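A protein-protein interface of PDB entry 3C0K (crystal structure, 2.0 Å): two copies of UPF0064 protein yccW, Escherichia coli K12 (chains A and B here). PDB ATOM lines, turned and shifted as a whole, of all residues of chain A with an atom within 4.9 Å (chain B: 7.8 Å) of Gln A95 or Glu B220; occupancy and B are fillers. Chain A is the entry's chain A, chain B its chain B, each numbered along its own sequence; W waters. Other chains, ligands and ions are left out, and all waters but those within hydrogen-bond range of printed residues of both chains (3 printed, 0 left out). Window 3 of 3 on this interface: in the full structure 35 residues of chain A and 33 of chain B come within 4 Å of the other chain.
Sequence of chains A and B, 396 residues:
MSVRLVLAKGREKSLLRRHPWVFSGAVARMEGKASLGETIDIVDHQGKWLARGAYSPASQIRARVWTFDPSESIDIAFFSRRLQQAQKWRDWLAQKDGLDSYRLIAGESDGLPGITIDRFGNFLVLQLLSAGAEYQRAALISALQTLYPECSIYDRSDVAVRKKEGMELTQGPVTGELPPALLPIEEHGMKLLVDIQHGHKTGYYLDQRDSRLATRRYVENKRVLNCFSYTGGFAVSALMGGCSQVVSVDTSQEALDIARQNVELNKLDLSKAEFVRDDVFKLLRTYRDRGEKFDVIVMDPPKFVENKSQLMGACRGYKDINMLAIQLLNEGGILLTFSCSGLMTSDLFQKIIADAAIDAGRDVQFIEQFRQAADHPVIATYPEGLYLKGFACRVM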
ATOM      1  N   ARG A  90       8.713  15.217  18.424  1.00  0.00           N
ATOM      2  CA  ARG A  90       7.478  15.713  17.821  1.00  0.00           C
ATOM      3  C   ARG A  90       7.238  17.199  18.026  1.00  0.00           C
ATOM      4  O   ARG A  90       6.546  17.826  17.225  1.00  0.00           O
ATOM      5  CB  ARG A  90       6.271  14.914  18.321  1.00  0.00           C
ATOM      6  CG  ARG A  90       6.095  13.574  17.614  1.00  0.00           C
ATOM      7  CD  ARG A  90       7.239  12.618  17.904  1.00  0.00           C
ATOM      8  NE  ARG A  90       7.031  11.310  17.292  1.00  0.00           N
ATOM      9  CZ  ARG A  90       7.727  10.220  17.599  1.00  0.00           C
ATOM     10  NH1 ARG A  90       8.681  10.273  18.517  1.00  0.00           N
ATOM     11  NH2 ARG A  90       7.468   9.070  16.991  1.00  0.00           N
ATOM     12  N   ASP A  91       7.791  17.769  19.092  1.00  0.00           N
ATOM     13  CA  ASP A  91       7.639  19.201  19.309  1.00  0.00           C
ATOM     14  C   ASP A  91       8.386  19.918  18.191  1.00  0.00           C
ATOM     15  O   ASP A  91       7.909  20.915  17.644  1.00  0.00           O
ATOM     16  CB  ASP A  91       8.212  19.625  20.669  1.00  0.00           C
ATOM     17  CG  ASP A  91       7.300  19.263  21.827  1.00  0.00           C
ATOM     18  OD1 ASP A  91       6.071  19.165  21.612  1.00  0.00           O
ATOM     19  OD2 ASP A  91       7.804  19.091  22.954  1.00  0.00           O
ATOM     20  N   TRP A  92       9.562  19.400  17.848  1.00  0.00           N
ATOM     21  CA  TRP A  92      10.370  19.988  16.781  1.00  0.00           C
ATOM     22  C   TRP A  92       9.697  19.823  15.416  1.00  0.00           C
ATOM     23  O   TRP A  92       9.665  20.755  14.610  1.00  0.00           O
ATOM     24  CB  TRP A  92      11.755  19.335  16.752  1.00  0.00           C
ATOM     25  CG  TRP A  92      12.681  19.985  15.777  1.00  0.00           C
ATOM     26  CD1 TRP A  92      13.496  21.056  16.007  1.00  0.00           C
ATOM     27  CD2 TRP A  92      12.833  19.655  14.394  1.00  0.00           C
ATOM     28  NE1 TRP A  92      14.144  21.417  14.851  1.00  0.00           N
ATOM     29  CE2 TRP A  92      13.756  20.572  13.845  1.00  0.00           C
ATOM     30  CE3 TRP A  92      12.274  18.676  13.563  1.00  0.00           C
ATOM     31  CZ2 TRP A  92      14.134  20.536  12.497  1.00  0.00           C
ATOM     32  CZ3 TRP A  92      12.647  18.643  12.226  1.00  0.00           C
ATOM     33  CH2 TRP A  92      13.570  19.569  11.707  1.00  0.00           C
ATOM     34  N   LEU A  93       9.159  18.634  15.158  1.00  0.00           N
ATOM     35  CA  LEU A  93       8.484  18.348  13.892  1.00  0.00           C
ATOM     36  C   LEU A  93       7.217  19.179  13.689  1.00  0.00           C
ATOM     37  O   LEU A  93       6.966  19.684  12.600  1.00  0.00           O
ATOM     38  CB  LEU A  93       8.103  16.863  13.809  1.00  0.00           C
ATOM     39  CG  LEU A  93       9.166  15.821  13.477  1.00  0.00           C
ATOM     40  CD1 LEU A  93       8.560  14.425  13.599  1.00  0.00           C
ATOM     41  CD2 LEU A  93       9.693  16.061  12.064  1.00  0.00           C
ATOM     42  N   ALA A  94       6.412  19.295  14.737  1.00  0.00           N
ATOM     43  CA  ALA A  94       5.160  20.041  14.670  1.00  0.00           C
ATOM     44  C   ALA A  94       5.382  21.514  14.362  1.00  0.00           C
ATOM     45  O   ALA A  94       4.666  22.102  13.552  1.00  0.00           O
ATOM     46  CB  ALA A  94       4.398  19.897  15.980  1.00  0.00           C
ATOM     47  N   GLN A  95       6.368  22.114  15.013  1.00  0.00           N
ATOM     48  CA  GLN A  95       6.645  23.522  14.779  1.00  0.00           C
ATOM     49  C   GLN A  95       7.232  23.693  13.377  1.00  0.00           C
ATOM     50  O   GLN A  95       6.887  24.632  12.662  1.00  0.00           O
ATOM     51  CB  GLN A  95       7.605  24.055  15.851  1.00  0.00           C
ATOM     52  CG  GLN A  95       9.073  24.115  15.449  1.00  0.00           C
ATOM     53  CD  GLN A  95       9.404  25.362  14.644  1.00  0.00           C
ATOM     54  OE1 GLN A  95      10.534  25.544  14.202  1.00  0.00           O
ATOM     55  NE2 GLN A  95       8.415  26.231  14.458  1.00  0.00           N
ATOM     56  N   LYS A  96       8.091  22.759  12.976  1.00  0.00           N
ATOM     57  CA  LYS A  96       8.731  22.826  11.669  1.00  0.00           C
ATOM     58  C   LYS A  96       7.782  22.564  10.497  1.00  0.00           C
ATOM     59  O   LYS A  96       7.864  23.243   9.476  1.00  0.00           O
ATOM     60  CB  LYS A  96       9.906  21.845  11.595  1.00  0.00           C
ATOM     61  CG  LYS A  96      10.822  22.080  10.402  1.00  0.00           C
ATOM     62  CD  LYS A  96      11.488  23.457  10.485  1.00  0.00           C
ATOM     63  CE  LYS A  96      12.275  23.791   9.223  1.00  0.00           C
ATOM     64  NZ  LYS A  96      12.857  25.177   9.271  1.00  0.00           N
ATOM     65  N   ASP A  97       6.879  21.595  10.637  1.00  0.00           N
ATOM     66  CA  ASP A  97       5.959  21.289   9.546  1.00  0.00           C
ATOM     67  C   ASP A  97       4.519  21.766   9.736  1.00  0.00           C
ATOM     68  O   ASP A  97       3.631  21.374   8.977  1.00  0.00           O
ATOM     69  CB  ASP A  97       5.979  19.783   9.248  1.00  0.00           C
ATOM     70  CG  ASP A  97       7.358  19.290   8.816  1.00  0.00           C
ATOM     71  OD1 ASP A  97       8.171  20.120   8.350  1.00  0.00           O
ATOM     72  OD2 ASP A  97       7.627  18.070   8.927  1.00  0.00           O
ATOM     73  N   GLY A  98       4.293  22.618  10.734  1.00  0.00           N
ATOM     74  CA  GLY A  98       2.960  23.147  10.992  1.00  0.00           C
ATOM     75  C   GLY A  98       1.920  22.096  11.334  1.00  0.00           C
ATOM     76  O   GLY A  98       0.847  22.054  10.735  1.00  0.00           O
ATOM     77  N   THR B 215      18.961  19.993   4.173  1.00  0.00           N
ATOM     78  CA  THR B 215      19.808  20.459   5.263  1.00  0.00           C
ATOM     79  C   THR B 215      19.223  21.736   5.868  1.00  0.00           C
ATOM     80  O   THR B 215      19.269  21.936   7.084  1.00  0.00           O
ATOM     81  CB  THR B 215      21.244  20.725   4.763  1.00  0.00           C
ATOM     82  OG1 THR B 215      21.790  19.509   4.235  1.00  0.00           O
ATOM     83  CG2 THR B 215      22.129  21.198   5.891  1.00  0.00           C
ATOM     84  N   ARG B 216      18.660  22.589   5.018  1.00  0.00           N
ATOM     85  CA  ARG B 216      18.067  23.844   5.477  1.00  0.00           C
ATOM     86  C   ARG B 216      17.000  23.651   6.559  1.00  0.00           C
ATOM     87  O   ARG B 216      16.943  24.402   7.525  1.00  0.00           O
ATOM     88  CB  ARG B 216      17.434  24.599   4.307  1.00  0.00           C
ATOM     89  CG  ARG B 216      18.367  24.903   3.166  1.00  0.00           C
ATOM     90  CD  ARG B 216      17.769  25.970   2.261  1.00  0.00           C
ATOM     91  NE  ARG B 216      18.479  26.047   0.990  1.00  0.00           N
ATOM     92  CZ  ARG B 216      18.105  26.818  -0.025  1.00  0.00           C
ATOM     93  NH1 ARG B 216      17.028  27.585   0.088  1.00  0.00           N
ATOM     94  NH2 ARG B 216      18.796  26.806  -1.159  1.00  0.00           N
ATOM     95  N   ARG B 217      16.160  22.638   6.388  1.00  0.00           N
ATOM     96  CA  ARG B 217      15.086  22.378   7.337  1.00  0.00           C
ATOM     97  C   ARG B 217      15.547  21.949   8.729  1.00  0.00           C
ATOM     98  O   ARG B 217      14.906  22.274   9.721  1.00  0.00           O
ATOM     99  CB  ARG B 217      14.133  21.331   6.748  1.00  0.00           C
ATOM    100  CG  ARG B 217      13.010  20.870   7.676  1.00  0.00           C
ATOM    101  CD  ARG B 217      11.876  20.215   6.886  1.00  0.00           C
ATOM    102  NE  ARG B 217      10.973  19.438   7.734  1.00  0.00           N
ATOM    103  CZ  ARG B 217      11.297  18.281   8.304  1.00  0.00           C
ATOM    104  NH1 ARG B 217      12.509  17.761   8.118  1.00  0.00           N
ATOM    105  NH2 ARG B 217      10.412  17.645   9.063  1.00  0.00           N
ATOM    106  N   TYR B 218      16.672  21.246   8.802  1.00  0.00           N
ATOM    107  CA  TYR B 218      17.182  20.743  10.077  1.00  0.00           C
ATOM    108  C   TYR B 218      18.058  21.656  10.914  1.00  0.00           C
ATOM    109  O   TYR B 218      18.217  21.423  12.104  1.00  0.00           O
ATOM    110  CB  TYR B 218      18.000  19.468   9.841  1.00  0.00           C
ATOM    111  CG  TYR B 218      17.213  18.266   9.396  1.00  0.00           C
ATOM    112  CD1 TYR B 218      16.333  17.627  10.263  1.00  0.00           C
ATOM    113  CD2 TYR B 218      17.380  17.741   8.113  1.00  0.00           C
ATOM    114  CE1 TYR B 218      15.637  16.481   9.865  1.00  0.00           C
ATOM    115  CE2 TYR B 218      16.690  16.607   7.706  1.00  0.00           C
ATOM    116  CZ  TYR B 218      15.821  15.981   8.588  1.00  0.00           C
ATOM    117  OH  TYR B 218      15.158  14.850   8.190  1.00  0.00           O
ATOM    118  N   VAL B 219      18.620  22.695  10.313  1.00  0.00           N
ATOM    119  CA  VAL B 219      19.585  23.518  11.024  1.00  0.00           C
ATOM    120  C   VAL B 219      19.220  24.815  11.741  1.00  0.00           C
ATOM    121  O   VAL B 219      20.116  25.468  12.272  1.00  0.00           O
ATOM    122  CB  VAL B 219      20.763  23.841  10.081  1.00  0.00           C
ATOM    123  CG1 VAL B 219      21.380  22.549   9.552  1.00  0.00           C
ATOM    124  CG2 VAL B 219      20.282  24.697   8.928  1.00  0.00           C
ATOM    125  N   GLU B 220      17.947  25.196  11.784  1.00  0.00           N
ATOM    126  CA  GLU B 220      17.601  26.454  12.435  1.00  0.00           C
ATOM    127  C   GLU B 220      18.161  26.623  13.847  1.00  0.00           C
ATOM    128  O   GLU B 220      17.882  25.825  14.738  1.00  0.00           O
ATOM    129  CB  GLU B 220      16.086  26.661  12.471  1.00  0.00           C
ATOM    130  CG  GLU B 220      15.701  27.975  13.130  1.00  0.00           C
ATOM    131  CD  GLU B 220      14.232  28.308  12.967  1.00  0.00           C
ATOM    132  OE1 GLU B 220      13.379  27.488  13.377  1.00  0.00           O
ATOM    133  OE2 GLU B 220      13.937  29.394  12.426  1.00  0.00           O
ATOM    134  N   ASN B 221      18.947  27.681  14.029  1.00  0.00           N
ATOM    135  CA  ASN B 221      19.569  28.004  15.309  1.00  0.00           C
ATOM    136  C   ASN B 221      20.398  26.862  15.894  1.00  0.00           C
ATOM    137  O   ASN B 221      20.585  26.773  17.109  1.00  0.00           O
ATOM    138  CB  ASN B 221      18.509  28.444  16.324  1.00  0.00           C
ATOM    139  CG  ASN B 221      17.798  29.717  15.904  1.00  0.00           C
ATOM    140  OD1 ASN B 221      18.422  30.645  15.393  1.00  0.00           O
ATOM    141  ND2 ASN B 221      16.488  29.774  16.131  1.00  0.00           N
ATOM    142  N   LYS B 222      20.915  25.999  15.028  1.00  0.00           N
ATOM    143  CA  LYS B 222      21.731  24.875  15.489  1.00  0.00           C
ATOM    144  C   LYS B 222      23.199  24.978  15.068  1.00  0.00           C
ATOM    145  O   LYS B 222      23.544  25.684  14.113  1.00  0.00           O
ATOM    146  CB  LYS B 222      21.149  23.559  14.969  1.00  0.00           C
ATOM    147  CG  LYS B 222      19.813  23.165  15.589  1.00  0.00           C
ATOM    148  CD  LYS B 222      19.300  21.871  14.962  1.00  0.00           C
ATOM    149  CE  LYS B 222      17.892  21.504  15.431  1.00  0.00           C
ATOM    150  NZ  LYS B 222      17.420  20.262  14.730  1.00  0.00           N
ATOM    151  N   ARG B 223      24.056  24.268  15.798  1.00  0.00           N
ATOM    152  CA  ARG B 223      25.483  24.221  15.512  1.00  0.00           C
ATOM    153  C   ARG B 223      25.701  23.057  14.539  1.00  0.00           C
ATOM    154  O   ARG B 223      25.378  21.904  14.852  1.00  0.00           O
ATOM    155  CB  ARG B 223      26.282  23.974  16.791  1.00  0.00           C
ATOM    156  CG  ARG B 223      27.770  24.170  16.591  1.00  0.00           C
ATOM    157  CD  ARG B 223      28.586  23.793  17.813  1.00  0.00           C
ATOM    158  NE  ARG B 223      29.962  24.261  17.653  1.00  0.00           N
ATOM    159  CZ  ARG B 223      31.026  23.676  18.195  1.00  0.00           C
ATOM    160  NH1 ARG B 223      30.883  22.591  18.944  1.00  0.00           N
ATOM    161  NH2 ARG B 223      32.235  24.177  17.981  1.00  0.00           N
ATOM    162  N   VAL B 224      26.260  23.361  13.373  1.00  0.00           N
ATOM    163  CA  VAL B 224      26.471  22.364  12.321  1.00  0.00           C
ATOM    164  C   VAL B 224      27.923  22.014  12.023  1.00  0.00           C
ATOM    165  O   VAL B 224      28.784  22.889  12.011  1.00  0.00           O
ATOM    166  CB  VAL B 224      25.860  22.867  10.984  1.00  0.00           C
ATOM    167  CG1 VAL B 224      25.931  21.777   9.915  1.00  0.00           C
ATOM    168  CG2 VAL B 224      24.437  23.353  11.218  1.00  0.00           C
ATOM    169  N   ALA B 238      23.325  25.308   5.115  1.00  0.00           N
ATOM    170  CA  ALA B 238      23.108  25.420   6.563  1.00  0.00           C
ATOM    171  C   ALA B 238      22.869  26.880   6.961  1.00  0.00           C
ATOM    172  O   ALA B 238      21.992  27.178   7.775  1.00  0.00           O
ATOM    173  CB  ALA B 238      24.304  24.859   7.340  1.00  0.00           C
ATOM    174  N   MET B 240      21.770  29.230   4.987  1.00  0.00           N
ATOM    175  CA  MET B 240      20.499  29.624   4.401  1.00  0.00           C
ATOM    176  C   MET B 240      19.379  29.184   5.345  1.00  0.00           C
ATOM    177  O   MET B 240      18.337  29.836   5.434  1.00  0.00           O
ATOM    178  CB  MET B 240      20.321  28.954   3.037  1.00  0.00           C
ATOM    179  CG  MET B 240      19.579  29.799   2.013  1.00  0.00           C
ATOM    180  SD  MET B 240      20.616  31.120   1.330  1.00  0.00           S
ATOM    181  CE  MET B 240      21.463  30.211   0.174  1.00  0.00           C
ATOM    182  N   GLY B 241      19.613  28.083   6.057  1.00  0.00           N
ATOM    183  CA  GLY B 241      18.630  27.558   6.990  1.00  0.00           C
ATOM    184  C   GLY B 241      18.648  28.230   8.356  1.00  0.00           C
ATOM    185  O   GLY B 241      17.862  27.879   9.242  1.00  0.00           O
ATOM    186  N   GLY B 242      19.552  29.186   8.537  1.00  0.00           N
ATOM    187  CA  GLY B 242      19.632  29.903   9.799  1.00  0.00           C
ATOM    188  C   GLY B 242      20.403  29.234  10.926  1.00  0.00           C
ATOM    189  O   GLY B 242      20.077  29.430  12.096  1.00  0.00           O
ATOM    190  N   CYS B 243      21.422  28.446  10.596  1.00  0.00           N
ATOM    191  CA  CYS B 243      22.211  27.786  11.634  1.00  0.00           C
ATOM    192  C   CYS B 243      22.942  28.845  12.472  1.00  0.00           C
ATOM    193  O   CYS B 243      23.258  29.929  11.977  1.00  0.00           O
ATOM    194  CB  CYS B 243      23.239  26.839  11.005  1.00  0.00           C
ATOM    195  SG  CYS B 243      24.539  27.667  10.037  1.00  0.00           S
ATOM    196  N   SER B 244      23.202  28.539  13.738  1.00  0.00           N
ATOM    197  CA  SER B 244      23.919  29.475  14.599  1.00  0.00           C
ATOM    198  C   SER B 244      25.397  29.477  14.214  1.00  0.00           C
ATOM    199  O   SER B 244      26.081  30.500  14.309  1.00  0.00           O
ATOM    200  CB  SER B 244      23.753  29.089  16.072  1.00  0.00           C
ATOM    201  OG  SER B 244      24.219  27.772  16.324  1.00  0.00           O
ATOM    202  N   ASP B 295      24.722  19.786  16.774  1.00  0.00           N
ATOM    203  CA  ASP B 295      23.303  19.449  16.664  1.00  0.00           C
ATOM    204  C   ASP B 295      23.032  18.761  15.333  1.00  0.00           C
ATOM    205  O   ASP B 295      22.150  17.906  15.229  1.00  0.00           O
ATOM    206  CB  ASP B 295      22.447  20.718  16.756  1.00  0.00           C
ATOM    207  CG  ASP B 295      22.704  21.501  18.028  1.00  0.00           C
ATOM    208  OD1 ASP B 295      22.610  20.898  19.120  1.00  0.00           O
ATOM    209  OD2 ASP B 295      22.995  22.714  17.937  1.00  0.00           O
ATOM    210  N   VAL B 296      23.799  19.144  14.317  1.00  0.00           N
ATOM    211  CA  VAL B 296      23.654  18.571  12.982  1.00  0.00           C
ATOM    212  C   VAL B 296      25.026  18.304  12.363  1.00  0.00           C
ATOM    213  O   VAL B 296      25.910  19.164  12.388  1.00  0.00           O
ATOM    214  CB  VAL B 296      22.862  19.519  12.040  1.00  0.00           C
ATOM    215  CG1 VAL B 296      22.793  18.921  10.635  1.00  0.00           C
ATOM    216  CG2 VAL B 296      21.443  19.743  12.579  1.00  0.00           C
HETATM  217  O   HOH W   1      15.624  18.564  16.092  1.00  0.00           O
HETATM  218  O   HOH W   2      15.645  23.839  14.748  1.00  0.00           O
HETATM  219  O   HOH W   3      15.513  26.149   8.951  1.00  0.00           O
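The side-chain carboxylate (OD2) of Asp A97 lies within salt-bridge range of the guanidinium group (NH2) of Arg B217, 2.8 Å away.
The side-chain amino group of Lys B222 lies close to the indole nitrogen of Trp A92 (3.5 Å).
O of Tyr B218 sits at hydrogen-bond distance from NZ of Lys B222 (3.0 Å).
The backbone carbonyl oxygen (O) of Lys B222 lies within hydrogen-bond range of the backbone NH (N) of Ser B244 (2.9 Å).
Arg B217 touches Trp A92 (O to CZ2, 3.4 Å).
CD1 of Tyr B218 touches CH2 of Trp A92 (3.7 Å).
Arg B217 touches Leu A93 (NH2 to CD2, 3.5 Å).
Glu B220 touches Gln A95.
Lys A96 touches Arg B217.
Printed residues of chain B within 4 Å of Trp A92: Arg B217 (3.4 Å), Tyr B218 (3.7 Å) and Lys B222 (3.5 Å).
Gln A95 touches just one residue of chain B: Glu B220.
Of the printed residues of chain B, Asp A97 touches Arg B217 (2.8 Å).
Thr B215 touches none of the printed residues of chain A.
Printed residues of chain A within 4 Å of Arg B217: Trp A92, Leu A93, Lys A96 and Asp A97.
Printed residues of chain A within 4 Å of Tyr B218: Trp A92.
Ala B238 touches none of the printed residues of chain A.
The nearest printed residue of chain A that does not touch Tyr B218 is Lys A96 (5.1 Å).
Of the 9 printed residues of chain A, 5 touch a printed residue of chain B.
Of the 18 printed residues of chain B, 4 touch a printed residue of chain A.
Hydrophobic or aromatic side chains of chain B within 4 Å of the printed part of chain A: Tyr B218.
Among the printed residues, Asp or Glu carboxylates within 4 Å of a Lys or Arg side-chain nitrogen of the other chain: Asp A97 with Arg B217.
No position is printed for both chains.
Water W3 lies within hydrogen-bond range of O of Arg B216 (2.7 Å), NZ of Lys A96 (2.8 Å) and O of Gly B241 (2.9 Å).
Water W1 bridges NZ of Lys B222 (2.8 Å) and NE1 of Trp A92 (3.4 Å).
Water W2 bridges the indole nitrogen of Trp A92 (2.9 Å) and the backbone carbonyl oxygen of Glu B220 (3.0 Å).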
